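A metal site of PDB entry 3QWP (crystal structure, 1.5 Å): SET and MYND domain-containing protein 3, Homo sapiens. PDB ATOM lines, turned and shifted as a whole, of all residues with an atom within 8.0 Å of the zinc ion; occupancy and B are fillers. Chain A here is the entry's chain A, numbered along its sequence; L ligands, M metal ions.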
ATOM      1  N   HIS A 207      24.000  23.720  -4.129  1.00  0.00           N
ATOM      2  CA  HIS A 207      24.903  23.647  -3.006  1.00  0.00           C
ATOM      3  C   HIS A 207      25.526  22.288  -2.773  1.00  0.00           C
ATOM      4  O   HIS A 207      24.855  21.266  -2.874  1.00  0.00           O
ATOM      5  CB  HIS A 207      24.093  24.031  -1.749  1.00  0.00           C
ATOM      6  CG  HIS A 207      24.826  23.740  -0.470  1.00  0.00           C
ATOM      7  ND1 HIS A 207      25.777  24.586   0.065  1.00  0.00           N
ATOM      8  CD2 HIS A 207      24.834  22.621   0.298  1.00  0.00           C
ATOM      9  CE1 HIS A 207      26.298  24.042   1.153  1.00  0.00           C
ATOM     10  NE2 HIS A 207      25.707  22.855   1.344  1.00  0.00           N
ATOM     11  N   SER A 208      26.784  22.303  -2.326  1.00  0.00           N
ATOM     12  CA  SER A 208      27.346  21.140  -1.649  1.00  0.00           C
ATOM     13  C   SER A 208      28.246  21.580  -0.531  1.00  0.00           C
ATOM     14  O   SER A 208      28.959  22.603  -0.637  1.00  0.00           O
ATOM     15  CB  SER A 208      28.196  20.393  -2.666  1.00  0.00           C
ATOM     16  OG  SER A 208      28.919  19.349  -2.023  1.00  0.00           O
ATOM     17  N   CYS A 209      28.243  20.770   0.554  1.00  0.00           N
ATOM     18  CA  CYS A 209      29.140  21.008   1.653  1.00  0.00           C
ATOM     19  C   CYS A 209      30.610  20.618   1.353  1.00  0.00           C
ATOM     20  O   CYS A 209      31.508  20.830   2.191  1.00  0.00           O
ATOM     21  CB  CYS A 209      28.628  20.189   2.875  1.00  0.00           C
ATOM     22  SG  CYS A 209      26.988  20.746   3.437  1.00  0.00           S
ATOM     23  N   ASP A 210      30.792  19.997   0.183  1.00  0.00           N
ATOM     24  CA  ASP A 210      32.122  19.644  -0.375  1.00  0.00           C
ATOM     25  C   ASP A 210      32.117  19.828  -1.886  1.00  0.00           C
ATOM     26  O   ASP A 210      31.967  18.863  -2.666  1.00  0.00           O
ATOM     27  CB  ASP A 210      32.477  18.205  -0.009  1.00  0.00           C
ATOM     28  CG  ASP A 210      33.804  17.781  -0.545  1.00  0.00           C
ATOM     29  OD1 ASP A 210      34.665  18.635  -0.885  1.00  0.00           O
ATOM     30  OD2 ASP A 210      34.028  16.549  -0.527  1.00  0.00           O
ATOM     31  N   CYS A 239      29.696  25.806  -2.404  1.00  0.00           N
ATOM     32  CA  CYS A 239      29.207  25.799  -1.038  1.00  0.00           C
ATOM     33  C   CYS A 239      28.568  27.158  -0.740  1.00  0.00           C
ATOM     34  O   CYS A 239      29.233  28.177  -0.760  1.00  0.00           O
ATOM     35  CB  CYS A 239      30.361  25.491  -0.086  1.00  0.00           C
ATOM     36  SG  CYS A 239      29.771  25.207   1.614  1.00  0.00           S
ATOM     37  N   LEU A 241      27.704  28.179   2.093  1.00  0.00           N
ATOM     38  CA  LEU A 241      27.871  28.466   3.516  1.00  0.00           C
ATOM     39  C   LEU A 241      29.348  28.648   3.904  1.00  0.00           C
ATOM     40  O   LEU A 241      30.267  28.022   3.336  1.00  0.00           O
ATOM     41  CB  LEU A 241      27.329  27.321   4.345  1.00  0.00           C
ATOM     42  CG  LEU A 241      25.881  27.004   4.042  1.00  0.00           C
ATOM     43  CD1 LEU A 241      25.498  25.830   4.940  1.00  0.00           C
ATOM     44  CD2 LEU A 241      25.028  28.204   4.259  1.00  0.00           C
ATOM     45  N   SER A 247      27.502  20.656  11.208  1.00  0.00           N
ATOM     46  CA  SER A 247      26.343  20.141  10.425  1.00  0.00           C
ATOM     47  C   SER A 247      25.007  20.635  10.970  1.00  0.00           C
ATOM     48  O   SER A 247      24.094  20.876  10.205  1.00  0.00           O
ATOM     49  CB  SER A 247      26.375  18.601  10.325  1.00  0.00           C
ATOM     50  OG  SER A 247      26.238  18.031  11.624  1.00  0.00           O
ATOM     51  N   ARG A 250      24.724  24.177   9.713  1.00  0.00           N
ATOM     52  CA  ARG A 250      24.445  24.177   8.235  1.00  0.00           C
ATOM     53  C   ARG A 250      22.965  23.788   8.030  1.00  0.00           C
ATOM     54  O   ARG A 250      22.282  24.359   7.195  1.00  0.00           O
ATOM     55  CB  ARG A 250      25.367  23.214   7.469  1.00  0.00           C
ATOM     56  CG  ARG A 250      26.838  23.610   7.563  1.00  0.00           C
ATOM     57  CD  ARG A 250      27.702  22.984   6.466  1.00  0.00           C
ATOM     58  NE  ARG A 250      27.624  21.513   6.464  1.00  0.00           N
ATOM     59  CZ  ARG A 250      28.352  20.705   7.245  1.00  0.00           C
ATOM     60  NH1 ARG A 250      29.163  21.230   8.151  1.00  0.00           N
ATOM     61  NH2 ARG A 250      28.201  19.384   7.183  1.00  0.00           N
ATOM     62  N   ARG A 251      22.507  22.782   8.766  1.00  0.00           N
ATOM     63  CA  ARG A 251      21.104  22.374   8.620  1.00  0.00           C
ATOM     64  C   ARG A 251      20.162  23.533   8.868  1.00  0.00           C
ATOM     65  O   ARG A 251      19.164  23.724   8.115  1.00  0.00           O
ATOM     66  CB  ARG A 251      20.811  21.213   9.617  1.00  0.00           C
ATOM     67  CG  ARG A 251      19.308  20.816   9.631  1.00  0.00           C
ATOM     68  CD  ARG A 251      19.061  19.537  10.524  1.00  0.00           C
ATOM     69  NE  ARG A 251      19.666  18.387   9.908  1.00  0.00           N
ATOM     70  CZ  ARG A 251      20.770  17.769  10.365  1.00  0.00           C
ATOM     71  NH1 ARG A 251      21.334  18.199  11.507  1.00  0.00           N
ATOM     72  NH2 ARG A 251      21.314  16.790   9.650  1.00  0.00           N
ATOM     73  N   LEU A 254      20.420  26.083   5.890  1.00  0.00           N
ATOM     74  CA  LEU A 254      19.904  25.544   4.613  1.00  0.00           C
ATOM     75  C   LEU A 254      18.393  25.410   4.684  1.00  0.00           C
ATOM     76  O   LEU A 254      17.717  25.726   3.702  1.00  0.00           O
ATOM     77  CB  LEU A 254      20.591  24.230   4.279  1.00  0.00           C
ATOM     78  CG  LEU A 254      22.106  24.381   4.058  1.00  0.00           C
ATOM     79  CD1 LEU A 254      22.626  22.987   3.768  1.00  0.00           C
ATOM     80  CD2 LEU A 254      22.441  25.342   2.907  1.00  0.00           C
ATOM     81  N   PHE A 260      15.953  23.632   1.997  1.00  0.00           N
ATOM     82  CA  PHE A 260      16.238  22.210   1.762  1.00  0.00           C
ATOM     83  C   PHE A 260      17.034  21.550   2.881  1.00  0.00           C
ATOM     84  O   PHE A 260      17.541  22.239   3.772  1.00  0.00           O
ATOM     85  CB  PHE A 260      16.889  21.975   0.396  1.00  0.00           C
ATOM     86  CG  PHE A 260      18.353  22.406   0.317  1.00  0.00           C
ATOM     87  CD1 PHE A 260      19.362  21.467   0.517  1.00  0.00           C
ATOM     88  CD2 PHE A 260      18.698  23.742   0.058  1.00  0.00           C
ATOM     89  CE1 PHE A 260      20.729  21.875   0.428  1.00  0.00           C
ATOM     90  CE2 PHE A 260      20.037  24.137  -0.034  1.00  0.00           C
ATOM     91  CZ  PHE A 260      21.048  23.208   0.135  1.00  0.00           C
ATOM     92  N   GLU A 261      17.014  20.216   2.833  1.00  0.00           N
ATOM     93  CA  GLU A 261      17.737  19.339   3.745  1.00  0.00           C
ATOM     94  C   GLU A 261      18.891  18.737   2.951  1.00  0.00           C
ATOM     95  O   GLU A 261      18.688  18.211   1.859  1.00  0.00           O
ATOM     96  CB  GLU A 261      16.778  18.204   4.198  1.00  0.00           C
ATOM     97  CG  GLU A 261      15.251  18.636   4.421  1.00  0.00           C
ATOM     98  CD  GLU A 261      15.104  19.524   5.613  1.00  0.00           C
ATOM     99  OE1 GLU A 261      16.097  19.585   6.403  1.00  0.00           O
ATOM    100  OE2 GLU A 261      14.001  20.119   5.840  1.00  0.00           O
ATOM    101  N   CYS A 262      20.127  19.050   3.342  1.00  0.00           N
ATOM    102  CA  CYS A 262      21.276  18.668   2.524  1.00  0.00           C
ATOM    103  C   CYS A 262      21.635  17.238   2.840  1.00  0.00           C
ATOM    104  O   CYS A 262      21.799  16.884   4.008  1.00  0.00           O
ATOM    105  CB  CYS A 262      22.486  19.591   2.825  1.00  0.00           C
ATOM    106  SG  CYS A 262      24.052  19.148   1.962  1.00  0.00           S
ATOM    107  N   ASP A 263      21.778  16.405   1.819  1.00  0.00           N
ATOM    108  CA  ASP A 263      22.154  15.037   2.096  1.00  0.00           C
ATOM    109  C   ASP A 263      23.531  14.609   1.564  1.00  0.00           C
ATOM    110  O   ASP A 263      23.749  13.440   1.279  1.00  0.00           O
ATOM    111  CB  ASP A 263      21.039  14.054   1.735  1.00  0.00           C
ATOM    112  CG  ASP A 263      21.022  13.714   0.289  1.00  0.00           C
ATOM    113  OD1 ASP A 263      21.448  14.563  -0.530  1.00  0.00           O
ATOM    114  OD2 ASP A 263      20.550  12.599  -0.051  1.00  0.00           O
ATOM    115  N   CYS A 264      24.488  15.534   1.566  1.00  0.00           N
ATOM    116  CA  CYS A 264      25.913  15.131   1.412  1.00  0.00           C
ATOM    117  C   CYS A 264      26.457  14.249   2.587  1.00  0.00           C
ATOM    118  O   CYS A 264      25.871  14.233   3.641  1.00  0.00           O
ATOM    119  CB  CYS A 264      26.803  16.363   1.122  1.00  0.00           C
ATOM    120  SG  CYS A 264      27.273  17.363   2.570  1.00  0.00           S
ATOM    121  N   PHE A 265      27.440  13.366   2.300  1.00  0.00           N
ATOM    122  CA  PHE A 265      28.231  12.589   3.219  1.00  0.00           C
ATOM    123  C   PHE A 265      28.608  13.362   4.478  1.00  0.00           C
ATOM    124  O   PHE A 265      28.574  12.800   5.567  1.00  0.00           O
ATOM    125  CB  PHE A 265      29.514  12.105   2.497  1.00  0.00           C
ATOM    126  CG  PHE A 265      30.521  11.456   3.427  1.00  0.00           C
ATOM    127  CD1 PHE A 265      30.292  10.170   3.960  1.00  0.00           C
ATOM    128  CD2 PHE A 265      31.641  12.169   3.871  1.00  0.00           C
ATOM    129  CE1 PHE A 265      31.189   9.588   4.888  1.00  0.00           C
ATOM    130  CE2 PHE A 265      32.523  11.606   4.817  1.00  0.00           C
ATOM    131  CZ  PHE A 265      32.325  10.292   5.284  1.00  0.00           C
ATOM    132  N   ARG A 266      29.011  14.637   4.326  1.00  0.00           N
ATOM    133  CA  ARG A 266      29.441  15.365   5.521  1.00  0.00           C
ATOM    134  C   ARG A 266      28.283  15.547   6.480  1.00  0.00           C
ATOM    135  O   ARG A 266      28.433  15.434   7.684  1.00  0.00           O
ATOM    136  CB  ARG A 266      30.028  16.728   5.156  1.00  0.00           C
ATOM    137  CG  ARG A 266      31.235  16.645   4.291  1.00  0.00           C
ATOM    138  CD  ARG A 266      31.977  17.984   4.205  1.00  0.00           C
ATOM    139  NE  ARG A 266      32.434  18.375   5.547  1.00  0.00           N
ATOM    140  CZ  ARG A 266      32.256  19.566   6.098  1.00  0.00           C
ATOM    141  NH1 ARG A 266      31.800  20.600   5.344  1.00  0.00           N
ATOM    142  NH2 ARG A 266      32.574  19.748   7.377  1.00  0.00           N
ATOM    143  N   CYS A 267      27.102  15.812   5.928  1.00  0.00           N
ATOM    144  CA  CYS A 267      25.941  15.992   6.817  1.00  0.00           C
ATOM    145  C   CYS A 267      25.475  14.660   7.446  1.00  0.00           C
ATOM    146  O   CYS A 267      25.185  14.612   8.612  1.00  0.00           O
ATOM    147  CB  CYS A 267      24.838  16.714   6.037  1.00  0.00           C
ATOM    148  SG  CYS A 267      25.273  18.453   5.702  1.00  0.00           S
ATOM    149  N   GLN A 268      25.509  13.538   6.738  1.00  0.00           N
ATOM    150  CA  GLN A 268      25.157  12.282   7.438  1.00  0.00           C
ATOM    151  C   GLN A 268      26.095  11.932   8.569  1.00  0.00           C
ATOM    152  O   GLN A 268      25.702  11.303   9.579  1.00  0.00           O
ATOM    153  CB  GLN A 268      25.072  11.100   6.486  1.00  0.00           C
ATOM    154  CG  GLN A 268      23.808  11.167   5.716  1.00  0.00           C
ATOM    155  CD  GLN A 268      23.403   9.871   5.053  1.00  0.00           C
ATOM    156  OE1 GLN A 268      23.324   8.819   5.710  1.00  0.00           O
ATOM    157  NE2 GLN A 268      22.987   9.970   3.791  1.00  0.00           N
HETATM  158  N1  LIG L   1      17.977  24.576  -7.985  1.00  0.00           N
HETATM  159  C1  LIG L   1      17.967  26.070  -8.234  1.00  0.00           C
HETATM  160  C2  LIG L   1      16.957  26.454  -9.292  1.00  0.00           C
HETATM  161  O1  LIG L   1      16.238  25.547  -9.752  1.00  0.00           O
HETATM  162  O2  LIG L   1      16.797  27.624  -9.654  1.00  0.00           O
HETATM  163  C3  LIG L   1      19.343  26.688  -8.465  1.00  0.00           C
HETATM  164  C4  LIG L   1      20.079  26.943  -7.111  1.00  0.00           C
HETATM  165  S1  LIG L   1      19.224  28.291  -6.192  1.00  0.00           S
HETATM  166  C5  LIG L   1      20.634  29.399  -5.892  1.00  0.00           C
HETATM  167  C6  LIG L   1      19.084  27.589  -4.520  1.00  0.00           C
HETATM  168  C7  LIG L   1      17.894  26.648  -4.406  1.00  0.00           C
HETATM  169  O3  LIG L   1      18.208  25.431  -5.063  1.00  0.00           O
HETATM  170  C8  LIG L   1      17.642  26.219  -2.960  1.00  0.00           C
HETATM  171  O4  LIG L   1      16.786  27.128  -2.277  1.00  0.00           O
HETATM  172  C9  LIG L   1      16.983  24.863  -3.156  1.00  0.00           C
HETATM  173  O5  LIG L   1      15.658  24.988  -3.713  1.00  0.00           O
HETATM  174  C10 LIG L   1      17.807  24.281  -4.309  1.00  0.00           C
HETATM  175  N2  LIG L   1      19.057  23.601  -3.825  1.00  0.00           N
HETATM  176  C11 LIG L   1      20.361  24.042  -3.931  1.00  0.00           C
HETATM  177  N3  LIG L   1      21.188  23.085  -3.519  1.00  0.00           N
HETATM  178  C12 LIG L   1      20.463  21.975  -3.203  1.00  0.00           C
HETATM  179  C13 LIG L   1      20.804  20.751  -2.670  1.00  0.00           C
HETATM  180  N4  LIG L   1      22.068  20.348  -2.449  1.00  0.00           N
HETATM  181  N5  LIG L   1      19.787  19.886  -2.377  1.00  0.00           N
HETATM  182  C14 LIG L   1      18.492  20.215  -2.590  1.00  0.00           C
HETATM  183  N6  LIG L   1      18.126  21.438  -3.086  1.00  0.00           N
HETATM  184  C15 LIG L   1      19.125  22.290  -3.380  1.00  0.00           C
HETATM  185 ZN    ZN M   1      25.746  18.627   3.427  1.00  0.00          ZN
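Four residues have an atom within 4 Å of the zinc ion: Cys 209, Cys 262, Cys 264 and Cys 267.
O of His 207 lies within hydrogen-bond range of N4 of the ligand, 3.0 Å away. N3 of the ligand is in hydrogen-bond range of N of His 207, at 2.9 Å.
The side-chain sulfur (SG) of Cys 264 binds the zinc ion (2.2 Å). The zinc ion is bound by SG of Cys 262, 2.3 Å away. The side-chain sulfur (SG) of Cys 267 binds the zinc ion, at 2.3 Å. SG of Cys 209 binds the zinc ion. The zinc ion has four donor atoms within binding distance.
The backbone NH of Cys 209 is in hydrogen-bond range of a ring nitrogen (NE2) of His 207 (3.4 Å). SG of Cys 209 sits close to NE of Arg 250 (3.2 Å). The backbone carbonyl oxygen of Cys 209 sits at hydrogen-bond distance from the guanidinium group of Arg 266 (3.2 Å). The guanidinium group of Arg 250 sits close to the side-chain sulfur of Cys 267, at 3.4 Å. The side-chain sulfur of Cys 264 lies close to the backbone NH of Arg 266 (3.7 Å).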
